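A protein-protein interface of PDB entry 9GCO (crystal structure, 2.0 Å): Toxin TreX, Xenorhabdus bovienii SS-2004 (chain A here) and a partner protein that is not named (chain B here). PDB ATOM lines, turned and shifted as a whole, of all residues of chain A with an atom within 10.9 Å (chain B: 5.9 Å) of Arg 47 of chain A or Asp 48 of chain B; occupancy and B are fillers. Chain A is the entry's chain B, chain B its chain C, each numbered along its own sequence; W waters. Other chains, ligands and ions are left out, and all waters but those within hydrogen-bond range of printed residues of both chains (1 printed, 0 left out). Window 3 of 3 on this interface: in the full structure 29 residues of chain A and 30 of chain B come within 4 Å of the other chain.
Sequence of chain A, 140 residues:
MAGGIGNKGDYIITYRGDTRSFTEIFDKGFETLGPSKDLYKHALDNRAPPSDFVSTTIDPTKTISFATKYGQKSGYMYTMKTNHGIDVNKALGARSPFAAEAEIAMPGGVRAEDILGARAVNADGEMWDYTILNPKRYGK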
ATOM      1  N   THR A  32      -3.177  21.963 -33.019  1.00  0.00           N
ATOM      2  CA  THR A  32      -1.902  21.429 -32.549  1.00  0.00           C
ATOM      3  C   THR A  32      -1.738  21.685 -31.046  1.00  0.00           C
ATOM      4  O   THR A  32      -2.471  22.473 -30.441  1.00  0.00           O
ATOM      5  CB  THR A  32      -0.716  22.072 -33.273  1.00  0.00           C
ATOM      6  OG1 THR A  32      -0.576  23.416 -32.792  1.00  0.00           O
ATOM      7  CG2 THR A  32      -0.919  22.088 -34.800  1.00  0.00           C
ATOM      8  N   LEU A  33      -0.715  21.049 -30.449  1.00  0.00           N
ATOM      9  CA  LEU A  33      -0.448  21.185 -29.017  1.00  0.00           C
ATOM     10  C   LEU A  33       0.835  21.944 -28.700  1.00  0.00           C
ATOM     11  O   LEU A  33       1.173  22.090 -27.522  1.00  0.00           O
ATOM     12  CB  LEU A  33      -0.383  19.794 -28.355  1.00  0.00           C
ATOM     13  CG  LEU A  33      -1.633  18.907 -28.466  1.00  0.00           C
ATOM     14  CD1 LEU A  33      -1.315  17.458 -28.105  1.00  0.00           C
ATOM     15  CD2 LEU A  33      -2.775  19.427 -27.561  1.00  0.00           C
ATOM     16  N   GLY A  34       1.582  22.405 -29.696  1.00  0.00           N
ATOM     17  CA  GLY A  34       2.852  23.050 -29.419  1.00  0.00           C
ATOM     18  C   GLY A  34       3.349  23.978 -30.507  1.00  0.00           C
ATOM     19  O   GLY A  34       2.754  24.092 -31.588  1.00  0.00           O
ATOM     20  N   PRO A  35       4.470  24.654 -30.237  1.00  0.00           N
ATOM     21  CA  PRO A  35       4.958  25.679 -31.173  1.00  0.00           C
ATOM     22  C   PRO A  35       6.086  25.230 -32.092  1.00  0.00           C
ATOM     23  O   PRO A  35       6.445  25.964 -33.021  1.00  0.00           O
ATOM     24  CB  PRO A  35       5.457  26.790 -30.224  1.00  0.00           C
ATOM     25  CG  PRO A  35       5.982  26.013 -29.070  1.00  0.00           C
ATOM     26  CD  PRO A  35       5.083  24.809 -28.898  1.00  0.00           C
ATOM     27  N   SER A  36       6.662  24.056 -31.851  1.00  0.00           N
ATOM     28  CA  SER A  36       7.859  23.667 -32.583  1.00  0.00           C
ATOM     29  C   SER A  36       7.541  23.330 -34.036  1.00  0.00           C
ATOM     30  O   SER A  36       6.694  22.466 -34.326  1.00  0.00           O
ATOM     31  CB  SER A  36       8.518  22.462 -31.937  1.00  0.00           C
ATOM     32  OG  SER A  36       9.684  22.144 -32.678  1.00  0.00           O
ATOM     33  N   ASP A  38       9.911  22.146 -36.134  1.00  0.00           N
ATOM     34  CA  ASP A  38      11.050  21.316 -36.538  1.00  0.00           C
ATOM     35  C   ASP A  38      10.512  19.927 -36.867  1.00  0.00           C
ATOM     36  O   ASP A  38      10.001  19.223 -35.986  1.00  0.00           O
ATOM     37  CB  ASP A  38      12.107  21.334 -35.425  1.00  0.00           C
ATOM     38  CG  ASP A  38      13.398  20.581 -35.796  1.00  0.00           C
ATOM     39  OD1 ASP A  38      13.326  19.594 -36.562  1.00  0.00           O
ATOM     40  OD2 ASP A  38      14.485  20.942 -35.271  1.00  0.00           O
ATOM     41  N   LEU A  39      10.543  19.568 -38.161  1.00  0.00           N
ATOM     42  CA  LEU A  39       9.933  18.326 -38.594  1.00  0.00           C
ATOM     43  C   LEU A  39      10.737  17.118 -38.138  1.00  0.00           C
ATOM     44  O   LEU A  39      10.155  16.074 -37.840  1.00  0.00           O
ATOM     45  CB  LEU A  39       9.778  18.326 -40.118  1.00  0.00           C
ATOM     46  CG  LEU A  39       8.865  17.215 -40.622  1.00  0.00           C
ATOM     47  CD1 LEU A  39       7.408  17.521 -40.316  1.00  0.00           C
ATOM     48  CD2 LEU A  39       9.066  16.994 -42.116  1.00  0.00           C
ATOM     49  N   TYR A  40      12.067  17.248 -38.094  1.00  0.00           N
ATOM     50  CA  TYR A  40      12.938  16.201 -37.572  1.00  0.00           C
ATOM     51  C   TYR A  40      12.608  15.893 -36.124  1.00  0.00           C
ATOM     52  O   TYR A  40      12.540  14.730 -35.732  1.00  0.00           O
ATOM     53  CB  TYR A  40      14.399  16.656 -37.744  1.00  0.00           C
ATOM     54  CG  TYR A  40      15.497  15.766 -37.183  1.00  0.00           C
ATOM     55  CD1 TYR A  40      15.902  15.872 -35.848  1.00  0.00           C
ATOM     56  CD2 TYR A  40      16.177  14.854 -37.999  1.00  0.00           C
ATOM     57  CE1 TYR A  40      16.911  15.065 -35.333  1.00  0.00           C
ATOM     58  CE2 TYR A  40      17.208  14.050 -37.484  1.00  0.00           C
ATOM     59  CZ  TYR A  40      17.568  14.168 -36.155  1.00  0.00           C
ATOM     60  OH  TYR A  40      18.574  13.377 -35.623  1.00  0.00           O
ATOM     61  N   LYS A  41      12.385  16.919 -35.310  1.00  0.00           N
ATOM     62  CA  LYS A  41      12.039  16.659 -33.918  1.00  0.00           C
ATOM     63  C   LYS A  41      10.616  16.175 -33.782  1.00  0.00           C
ATOM     64  O   LYS A  41      10.330  15.415 -32.856  1.00  0.00           O
ATOM     65  CB  LYS A  41      12.256  17.916 -33.069  1.00  0.00           C
ATOM     66  CG  LYS A  41      13.703  18.349 -32.984  1.00  0.00           C
ATOM     67  CD  LYS A  41      13.878  19.563 -32.024  1.00  0.00           C
ATOM     68  CE  LYS A  41      15.283  20.132 -32.088  1.00  0.00           C
ATOM     69  NZ  LYS A  41      15.569  21.037 -30.929  1.00  0.00           N
ATOM     70  N   HIS A  42       9.723  16.585 -34.698  1.00  0.00           N
ATOM     71  CA  HIS A  42       8.365  16.044 -34.709  1.00  0.00           C
ATOM     72  C   HIS A  42       8.381  14.535 -34.905  1.00  0.00           C
ATOM     73  O   HIS A  42       7.617  13.811 -34.256  1.00  0.00           O
ATOM     74  CB  HIS A  42       7.540  16.720 -35.807  1.00  0.00           C
ATOM     75  CG  HIS A  42       6.260  16.017 -36.122  1.00  0.00           C
ATOM     76  ND1 HIS A  42       5.073  16.295 -35.473  1.00  0.00           N
ATOM     77  CD2 HIS A  42       5.985  15.037 -37.014  1.00  0.00           C
ATOM     78  CE1 HIS A  42       4.126  15.505 -35.949  1.00  0.00           C
ATOM     79  NE2 HIS A  42       4.650  14.743 -36.894  1.00  0.00           N
ATOM     80  N   ALA A  43       9.244  14.049 -35.811  1.00  0.00           N
ATOM     81  CA  ALA A  43       9.311  12.624 -36.111  1.00  0.00           C
ATOM     82  C   ALA A  43       9.930  11.832 -34.961  1.00  0.00           C
ATOM     83  O   ALA A  43       9.428  10.764 -34.605  1.00  0.00           O
ATOM     84  CB  ALA A  43      10.126  12.418 -37.393  1.00  0.00           C
ATOM     85  N   LEU A  44      11.002  12.350 -34.361  1.00  0.00           N
ATOM     86  CA  LEU A  44      11.617  11.686 -33.214  1.00  0.00           C
ATOM     87  C   LEU A  44      10.630  11.557 -32.057  1.00  0.00           C
ATOM     88  O   LEU A  44      10.435  10.468 -31.505  1.00  0.00           O
ATOM     89  CB  LEU A  44      12.859  12.462 -32.784  1.00  0.00           C
ATOM     90  CG  LEU A  44      13.551  12.051 -31.467  1.00  0.00           C
ATOM     91  CD1 LEU A  44      13.811  10.554 -31.415  1.00  0.00           C
ATOM     92  CD2 LEU A  44      14.807  12.839 -31.287  1.00  0.00           C
ATOM     93  N   ASP A  45       9.980  12.658 -31.690  1.00  0.00           N
ATOM     94  CA  ASP A  45       9.141  12.724 -30.510  1.00  0.00           C
ATOM     95  C   ASP A  45       8.338  14.003 -30.563  1.00  0.00           C
ATOM     96  O   ASP A  45       8.858  15.076 -30.249  1.00  0.00           O
ATOM     97  CB  ASP A  45       9.993  12.680 -29.213  1.00  0.00           C
ATOM     98  CG  ASP A  45       9.120  12.585 -27.974  1.00  0.00           C
ATOM     99  OD1 ASP A  45       7.912  12.854 -28.122  1.00  0.00           O
ATOM    100  OD2 ASP A  45       9.596  12.212 -26.892  1.00  0.00           O
ATOM    101  N   ASN A  46       7.080  13.931 -31.002  1.00  0.00           N
ATOM    102  CA  ASN A  46       6.278  15.120 -31.236  1.00  0.00           C
ATOM    103  C   ASN A  46       5.711  15.693 -29.945  1.00  0.00           C
ATOM    104  O   ASN A  46       4.975  16.681 -29.994  1.00  0.00           O
ATOM    105  CB  ASN A  46       5.144  14.836 -32.242  1.00  0.00           C
ATOM    106  CG  ASN A  46       4.116  13.843 -31.728  1.00  0.00           C
ATOM    107  OD1 ASN A  46       4.426  12.941 -30.952  1.00  0.00           O
ATOM    108  ND2 ASN A  46       2.866  13.996 -32.204  1.00  0.00           N
ATOM    109  N   ARG A  47       6.063  15.133 -28.797  1.00  0.00           N
ATOM    110  CA  ARG A  47       5.704  15.701 -27.508  1.00  0.00           C
ATOM    111  C   ARG A  47       6.894  16.301 -26.780  1.00  0.00           C
ATOM    112  O   ARG A  47       6.710  16.921 -25.722  1.00  0.00           O
ATOM    113  CB  ARG A  47       5.045  14.629 -26.624  1.00  0.00           C
ATOM    114  CG  ARG A  47       4.126  15.223 -25.574  1.00  0.00           C
ATOM    115  CD  ARG A  47       4.086  14.380 -24.336  1.00  0.00           C
ATOM    116  NE  ARG A  47       3.445  15.087 -23.232  1.00  0.00           N
ATOM    117  CZ  ARG A  47       4.001  16.094 -22.567  1.00  0.00           C
ATOM    118  NH1 ARG A  47       5.183  16.584 -22.909  1.00  0.00           N
ATOM    119  NH2 ARG A  47       3.356  16.625 -21.530  1.00  0.00           N
ATOM    120  N   ALA A  48       8.103  16.169 -27.326  1.00  0.00           N
ATOM    121  CA  ALA A  48       9.307  16.693 -26.676  1.00  0.00           C
ATOM    122  C   ALA A  48      10.300  17.149 -27.735  1.00  0.00           C
ATOM    123  O   ALA A  48      11.139  16.365 -28.203  1.00  0.00           O
ATOM    124  CB  ALA A  48       9.944  15.638 -25.774  1.00  0.00           C
ATOM    125  N   PRO A  49      10.235  18.424 -28.150  1.00  0.00           N
ATOM    126  CA  PRO A  49       9.260  19.459 -27.764  1.00  0.00           C
ATOM    127  C   PRO A  49       7.911  19.253 -28.471  1.00  0.00           C
ATOM    128  O   PRO A  49       7.822  18.702 -29.567  1.00  0.00           O
ATOM    129  CB  PRO A  49       9.966  20.767 -28.183  1.00  0.00           C
ATOM    130  CG  PRO A  49      10.790  20.363 -29.391  1.00  0.00           C
ATOM    131  CD  PRO A  49      11.276  18.958 -29.059  1.00  0.00           C
ATOM    132  N   PRO A  50       6.817  19.682 -27.847  1.00  0.00           N
ATOM    133  CA  PRO A  50       5.507  19.571 -28.499  1.00  0.00           C
ATOM    134  C   PRO A  50       5.499  20.334 -29.820  1.00  0.00           C
ATOM    135  O   PRO A  50       5.930  21.486 -29.896  1.00  0.00           O
ATOM    136  CB  PRO A  50       4.553  20.184 -27.467  1.00  0.00           C
ATOM    137  CG  PRO A  50       5.394  21.125 -26.721  1.00  0.00           C
ATOM    138  CD  PRO A  50       6.730  20.434 -26.580  1.00  0.00           C
ATOM    139  N   SER A  51       5.034  19.674 -30.870  1.00  0.00           N
ATOM    140  CA  SER A  51       5.227  20.171 -32.224  1.00  0.00           C
ATOM    141  C   SER A  51       3.970  20.879 -32.734  1.00  0.00           C
ATOM    142  O   SER A  51       2.841  20.597 -32.314  1.00  0.00           O
ATOM    143  CB  SER A  51       5.598  19.006 -33.156  1.00  0.00           C
ATOM    144  OG  SER A  51       4.441  18.306 -33.624  1.00  0.00           O
ATOM    145  N   ASP A  52       4.177  21.787 -33.690  1.00  0.00           N
ATOM    146  CA  ASP A  52       3.053  22.501 -34.308  1.00  0.00           C
ATOM    147  C   ASP A  52       2.564  21.808 -35.582  1.00  0.00           C
ATOM    148  O   ASP A  52       2.308  22.450 -36.602  1.00  0.00           O
ATOM    149  CB  ASP A  52       3.463  23.947 -34.571  1.00  0.00           C
ATOM    150  CG  ASP A  52       2.254  24.879 -34.737  1.00  0.00           C
ATOM    151  OD1 ASP A  52       1.109  24.470 -34.464  1.00  0.00           O
ATOM    152  OD2 ASP A  52       2.447  26.006 -35.176  1.00  0.00           O
ATOM    153  N   PHE A  53       2.383  20.492 -35.513  1.00  0.00           N
ATOM    154  CA  PHE A  53       1.835  19.722 -36.621  1.00  0.00           C
ATOM    155  C   PHE A  53       0.690  18.830 -36.158  1.00  0.00           C
ATOM    156  O   PHE A  53       0.712  18.302 -35.040  1.00  0.00           O
ATOM    157  CB  PHE A  53       2.890  18.825 -37.280  1.00  0.00           C
ATOM    158  CG  PHE A  53       4.110  19.555 -37.760  1.00  0.00           C
ATOM    159  CD1 PHE A  53       4.133  20.119 -39.022  1.00  0.00           C
ATOM    160  CD2 PHE A  53       5.221  19.663 -36.970  1.00  0.00           C
ATOM    161  CE1 PHE A  53       5.251  20.772 -39.473  1.00  0.00           C
ATOM    162  CE2 PHE A  53       6.340  20.334 -37.404  1.00  0.00           C
ATOM    163  CZ  PHE A  53       6.364  20.888 -38.656  1.00  0.00           C
ATOM    164  N   SER A  55      -1.029  15.287 -37.409  1.00  0.00           N
ATOM    165  CA  SER A  55      -0.724  14.147 -38.283  1.00  0.00           C
ATOM    166  C   SER A  55      -1.964  13.715 -39.066  1.00  0.00           C
ATOM    167  O   SER A  55      -3.054  13.599 -38.481  1.00  0.00           O
ATOM    168  CB  SER A  55      -0.196  12.944 -37.482  1.00  0.00           C
ATOM    169  OG  SER A  55       1.056  13.225 -36.890  1.00  0.00           O
ATOM    170  N   LYS A  69      -8.300   2.318 -31.155  1.00  0.00           N
ATOM    171  CA  LYS A  69      -7.388   1.976 -30.054  1.00  0.00           C
ATOM    172  C   LYS A  69      -7.107   0.473 -30.040  1.00  0.00           C
ATOM    173  O   LYS A  69      -7.246  -0.214 -29.022  1.00  0.00           O
ATOM    174  CB  LYS A  69      -7.955   2.466 -28.723  1.00  0.00           C
ATOM    175  CG  LYS A  69      -8.207   3.986 -28.772  1.00  0.00           C
ATOM    176  CD  LYS A  69      -8.322   4.633 -27.409  1.00  0.00           C
ATOM    177  CE  LYS A  69      -8.475   6.162 -27.590  1.00  0.00           C
ATOM    178  NZ  LYS A  69      -7.959   6.841 -26.397  1.00  0.00           N
ATOM    179  N   GLU A 103       2.526   9.672 -43.844  1.00  0.00           N
ATOM    180  CA  GLU A 103       2.084  10.798 -43.030  1.00  0.00           C
ATOM    181  C   GLU A 103       2.215  12.114 -43.787  1.00  0.00           C
ATOM    182  O   GLU A 103       3.257  12.396 -44.407  1.00  0.00           O
ATOM    183  CB  GLU A 103       2.914  10.857 -41.742  1.00  0.00           C
ATOM    184  CG  GLU A 103       2.443  11.888 -40.695  1.00  0.00           C
ATOM    185  CD  GLU A 103       3.414  12.077 -39.501  1.00  0.00           C
ATOM    186  OE1 GLU A 103       4.407  11.331 -39.390  1.00  0.00           O
ATOM    187  OE2 GLU A 103       3.194  13.016 -38.676  1.00  0.00           O
ATOM    188  N   ARG B  30      -8.491  17.701 -24.774  1.00  0.00           N
ATOM    189  CA  ARG B  30      -7.443  16.698 -24.924  1.00  0.00           C
ATOM    190  C   ARG B  30      -6.841  16.292 -23.585  1.00  0.00           C
ATOM    191  O   ARG B  30      -5.688  15.866 -23.506  1.00  0.00           O
ATOM    192  CB  ARG B  30      -6.330  17.182 -25.853  1.00  0.00           C
ATOM    193  CG  ARG B  30      -6.762  17.506 -27.268  1.00  0.00           C
ATOM    194  CD  ARG B  30      -6.823  16.228 -28.082  1.00  0.00           C
ATOM    195  NE  ARG B  30      -5.535  15.854 -28.655  1.00  0.00           N
ATOM    196  CZ  ARG B  30      -4.927  16.487 -29.647  1.00  0.00           C
ATOM    197  NH1 ARG B  30      -5.366  17.647 -30.104  1.00  0.00           N
ATOM    198  NH2 ARG B  30      -3.845  15.939 -30.190  1.00  0.00           N
ATOM    199  N   HIS B  31      -7.615  16.401 -22.524  1.00  0.00           N
ATOM    200  CA  HIS B  31      -7.135  16.104 -21.191  1.00  0.00           C
ATOM    201  C   HIS B  31      -7.284  14.601 -20.958  1.00  0.00           C
ATOM    202  O   HIS B  31      -8.400  14.084 -20.865  1.00  0.00           O
ATOM    203  CB  HIS B  31      -7.897  16.945 -20.169  1.00  0.00           C
ATOM    204  CG  HIS B  31      -7.431  16.729 -18.768  1.00  0.00           C
ATOM    205  ND1 HIS B  31      -8.277  16.326 -17.759  1.00  0.00           N
ATOM    206  CD2 HIS B  31      -6.199  16.833 -18.211  1.00  0.00           C
ATOM    207  CE1 HIS B  31      -7.590  16.197 -16.635  1.00  0.00           C
ATOM    208  NE2 HIS B  31      -6.326  16.497 -16.882  1.00  0.00           N
ATOM    209  N   CYS B  32      -6.156  13.895 -20.913  1.00  0.00           N
ATOM    210  CA  CYS B  32      -6.125  12.478 -20.583  1.00  0.00           C
ATOM    211  C   CYS B  32      -5.724  12.312 -19.125  1.00  0.00           C
ATOM    212  O   CYS B  32      -4.717  12.882 -18.697  1.00  0.00           O
ATOM    213  CB  CYS B  32      -5.140  11.723 -21.471  1.00  0.00           C
ATOM    214  SG  CYS B  32      -5.513  11.853 -23.252  1.00  0.00           S
ATOM    215  N   CYS B  33      -6.496  11.517 -18.381  1.00  0.00           N
ATOM    216  CA  CYS B  33      -6.224  11.213 -16.978  1.00  0.00           C
ATOM    217  C   CYS B  33      -6.105   9.705 -16.790  1.00  0.00           C
ATOM    218  O   CYS B  33      -6.938   8.939 -17.290  1.00  0.00           O
ATOM    219  CB  CYS B  33      -7.314  11.750 -16.048  1.00  0.00           C
ATOM    220  SG  CYS B  33      -7.049  11.276 -14.297  1.00  0.00           S
ATOM    221  N   SER B  46      -1.949  10.454 -13.075  1.00  0.00           N
ATOM    222  CA  SER B  46      -1.184  11.369 -13.903  1.00  0.00           C
ATOM    223  C   SER B  46      -2.114  11.957 -14.949  1.00  0.00           C
ATOM    224  O   SER B  46      -3.079  11.312 -15.369  1.00  0.00           O
ATOM    225  CB  SER B  46      -0.004  10.674 -14.603  1.00  0.00           C
ATOM    226  OG  SER B  46       0.700  11.594 -15.444  1.00  0.00           O
ATOM    227  N   ASN B  47      -1.818  13.190 -15.363  1.00  0.00           N
ATOM    228  CA  ASN B  47      -2.579  13.891 -16.390  1.00  0.00           C
ATOM    229  C   ASN B  47      -1.613  14.331 -17.483  1.00  0.00           C
ATOM    230  O   ASN B  47      -0.455  14.671 -17.197  1.00  0.00           O
ATOM    231  CB  ASN B  47      -3.326  15.110 -15.810  1.00  0.00           C
ATOM    232  CG  ASN B  47      -4.218  14.741 -14.635  1.00  0.00           C
ATOM    233  OD1 ASN B  47      -5.379  14.375 -14.814  1.00  0.00           O
ATOM    234  ND2 ASN B  47      -3.678  14.829 -13.429  1.00  0.00           N
ATOM    235  N   ASP B  48      -2.081  14.279 -18.727  1.00  0.00           N
ATOM    236  CA  ASP B  48      -1.301  14.688 -19.898  1.00  0.00           C
ATOM    237  C   ASP B  48      -2.250  14.790 -21.096  1.00  0.00           C
ATOM    238  O   ASP B  48      -3.475  14.713 -20.940  1.00  0.00           O
ATOM    239  CB  ASP B  48      -0.141  13.714 -20.140  1.00  0.00           C
ATOM    240  CG  ASP B  48       1.012  14.379 -20.870  1.00  0.00           C
ATOM    241  OD1 ASP B  48       0.884  14.660 -22.090  1.00  0.00           O
ATOM    242  OD2 ASP B  48       2.033  14.661 -20.213  1.00  0.00           O
ATOM    243  N   THR B  49      -1.681  14.935 -22.305  1.00  0.00           N
ATOM    244  CA  THR B  49      -2.461  15.029 -23.533  1.00  0.00           C
ATOM    245  C   THR B  49      -2.458  13.734 -24.326  1.00  0.00           C
ATOM    246  O   THR B  49      -3.067  13.684 -25.390  1.00  0.00           O
ATOM    247  CB  THR B  49      -1.952  16.175 -24.442  1.00  0.00           C
ATOM    248  OG1 THR B  49      -0.522  16.138 -24.538  1.00  0.00           O
ATOM    249  CG2 THR B  49      -2.362  17.529 -23.891  1.00  0.00           C
ATOM    250  N   ASP B  50      -1.764  12.701 -23.852  1.00  0.00           N
ATOM    251  CA  ASP B  50      -1.864  11.353 -24.417  1.00  0.00           C
ATOM    252  C   ASP B  50      -1.519  10.362 -23.313  1.00  0.00           C
ATOM    253  O   ASP B  50      -0.841  10.718 -22.340  1.00  0.00           O
ATOM    254  CB  ASP B  50      -0.929  11.168 -25.613  1.00  0.00           C
ATOM    255  CG  ASP B  50       0.539  11.046 -25.189  1.00  0.00           C
ATOM    256  OD1 ASP B  50       0.968   9.935 -24.817  1.00  0.00           O
ATOM    257  OD2 ASP B  50       1.268  12.062 -25.223  1.00  0.00           O
ATOM    258  N   SER B  53       2.301   9.277 -22.442  1.00  0.00           N
ATOM    259  CA  SER B  53       2.905  10.217 -21.497  1.00  0.00           C
ATOM    260  C   SER B  53       2.357  10.027 -20.089  1.00  0.00           C
ATOM    261  O   SER B  53       3.118  10.060 -19.120  1.00  0.00           O
ATOM    262  CB  SER B  53       2.669  11.646 -21.958  1.00  0.00           C
ATOM    263  OG  SER B  53       3.331  11.893 -23.183  1.00  0.00           O
ATOM    264  N   CYS B  54       1.036   9.874 -19.943  1.00  0.00           N
ATOM    265  CA  CYS B  54       0.474   9.625 -18.618  1.00  0.00           C
ATOM    266  C   CYS B  54       1.165   8.425 -17.974  1.00  0.00           C
ATOM    267  O   CYS B  54       1.548   8.462 -16.801  1.00  0.00           O
ATOM    268  CB  CYS B  54      -1.031   9.354 -18.696  1.00  0.00           C
ATOM    269  SG  CYS B  54      -2.144  10.711 -19.138  1.00  0.00           S
ATOM    270  N   ASP B  57       4.707   8.968 -16.839  1.00  0.00           N
ATOM    271  CA  ASP B  57       4.683   9.772 -15.613  1.00  0.00           C
ATOM    272  C   ASP B  57       4.235   8.926 -14.429  1.00  0.00           C
ATOM    273  O   ASP B  57       4.800   9.028 -13.338  1.00  0.00           O
ATOM    274  CB  ASP B  57       3.759  10.978 -15.856  1.00  0.00           C
ATOM    275  CG  ASP B  57       3.647  11.928 -14.666  1.00  0.00           C
ATOM    276  OD1 ASP B  57       4.312  11.737 -13.627  1.00  0.00           O
ATOM    277  OD2 ASP B  57       2.865  12.902 -14.802  1.00  0.00           O
ATOM    278  N   ARG B  83       0.560   8.554 -31.489  1.00  0.00           N
ATOM    279  CA  ARG B  83       0.317   9.350 -30.292  1.00  0.00           C
ATOM    280  C   ARG B  83      -0.862  10.276 -30.526  1.00  0.00           C
ATOM    281  O   ARG B  83      -1.800  10.329 -29.728  1.00  0.00           O
ATOM    282  CB  ARG B  83       1.573  10.153 -29.928  1.00  0.00           C
ATOM    283  CG  ARG B  83       1.484  10.903 -28.579  1.00  0.00           C
ATOM    284  CD  ARG B  83       2.689  11.870 -28.304  1.00  0.00           C
ATOM    285  NE  ARG B  83       4.018  11.258 -28.321  1.00  0.00           N
ATOM    286  CZ  ARG B  83       4.658  10.760 -27.264  1.00  0.00           C
ATOM    287  NH1 ARG B  83       4.092  10.690 -26.066  1.00  0.00           N
ATOM    288  NH2 ARG B  83       5.899  10.322 -27.416  1.00  0.00           N
HETATM  289  O   HOH W   1       6.079  10.189 -30.183  1.00  0.00           O
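The side-chain carboxylate (OD1) of Asp 45 of chain A lies within salt-bridge range of the guanidinium group (NH2) of Arg 83 of chain B, at 3.3 Å. OD1 of Asn 46 of chain A is in hydrogen-bond range of NE of Arg 83 of chain B (3.1 Å). NE of Arg 47 of chain A lies within salt-bridge range of OD1 of Asp 48 of chain B (2.8 Å). NE of Arg 47 of chain A lies close to OG of Ser 53 of chain B (3.2 Å).
The side-chain carboxylate (OD1) of Asp 45 of chain A is in hydrogen-bond range of the backbone NH (N) of Arg 47 of chain A, at 3.0 Å. OD1 of Asp 45 of chain A sits at hydrogen-bond distance from N of Ala 48 of chain A (3.4 Å). The side-chain sulfur of Cys 54 of chain B is in hydrogen-bond range of the backbone NH of Asp 48 of chain B, 3.6 Å away. The side-chain sulfur (SG) of Cys 54 of chain B sits at hydrogen-bond distance from the backbone carbonyl oxygen (O) of Asp 50 of chain B (3.5 Å). The side-chain carboxylate of Asp 50 of chain B is in salt-bridge range of the guanidinium group of Arg 83 of chain B (3.3 Å). NH1 of Arg 83 of chain B lies within hydrogen-bond range of OG of Ser 53 of chain B (3.2 Å).
Among the printed residues, merely in contact across the chains: Leu 33 of chain A with Arg 30 of chain B (3.6 Å), Leu 33 of chain A with Thr 49 of chain B (3.9 Å), Arg 47 of chain A with Asp 50 of chain B (3.8 Å) and Arg 47 of chain A with Arg 83 of chain B (3.9 Å).
Of chain A, only Arg 47 comes within 4 Å of Asp 48 of chain B. No residue of chain A comes within 4 Å of His 31 of chain B. No residue of chain A comes within 4 Å of Cys 32 of chain B. Asn 47 of chain B touches none of the printed residues of chain A. Asp 50 of chain B touches just one residue of chain A: Arg 47 (3.8 Å). Of chain A, only Arg 47 (2.8 Å) comes within 4 Å of Ser 53 of chain B. Cys 54 of chain B touches none of the printed residues of chain A. Of the printed residues of chain A, Arg 83 of chain B touches Asp 45 (3.3 Å), Asn 46 (3.1 Å) and Arg 47 (3.9 Å). Printed residues of chain B within 4 Å of Asp 45 of chain A: Arg 83. Of the printed residues of chain B, Asn 46 of chain A touches Arg 83. Ser 36 of chain A touches none of the printed residues of chain B. Leu 44 of chain A touches none of the printed residues of chain B. The nearest residue of chain B that does not touch Arg 47 of chain A is Thr 49 of chain B (4.3 Å). The nearest residue of chain A that does not touch Asp 48 of chain B is Leu 33 of chain A (7.0 Å). The nearest printed residue of chain B that does not touch Asn 46 of chain A is Asp 50 of chain B (6.6 Å).
Among the printed residues, Asp or Glu carboxylates within 4 Å of a Lys or Arg side-chain nitrogen of the other chain: Asp 45 of chain A with Arg 83 of chain B and Arg 47 of chain A with Asp 48 of chain B.
Water W1 bridges the guanidinium group of Arg 83 of chain B (2.8 Å) and the side-chain amide oxygen of Asn 46 of chain A (3.3 Å).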
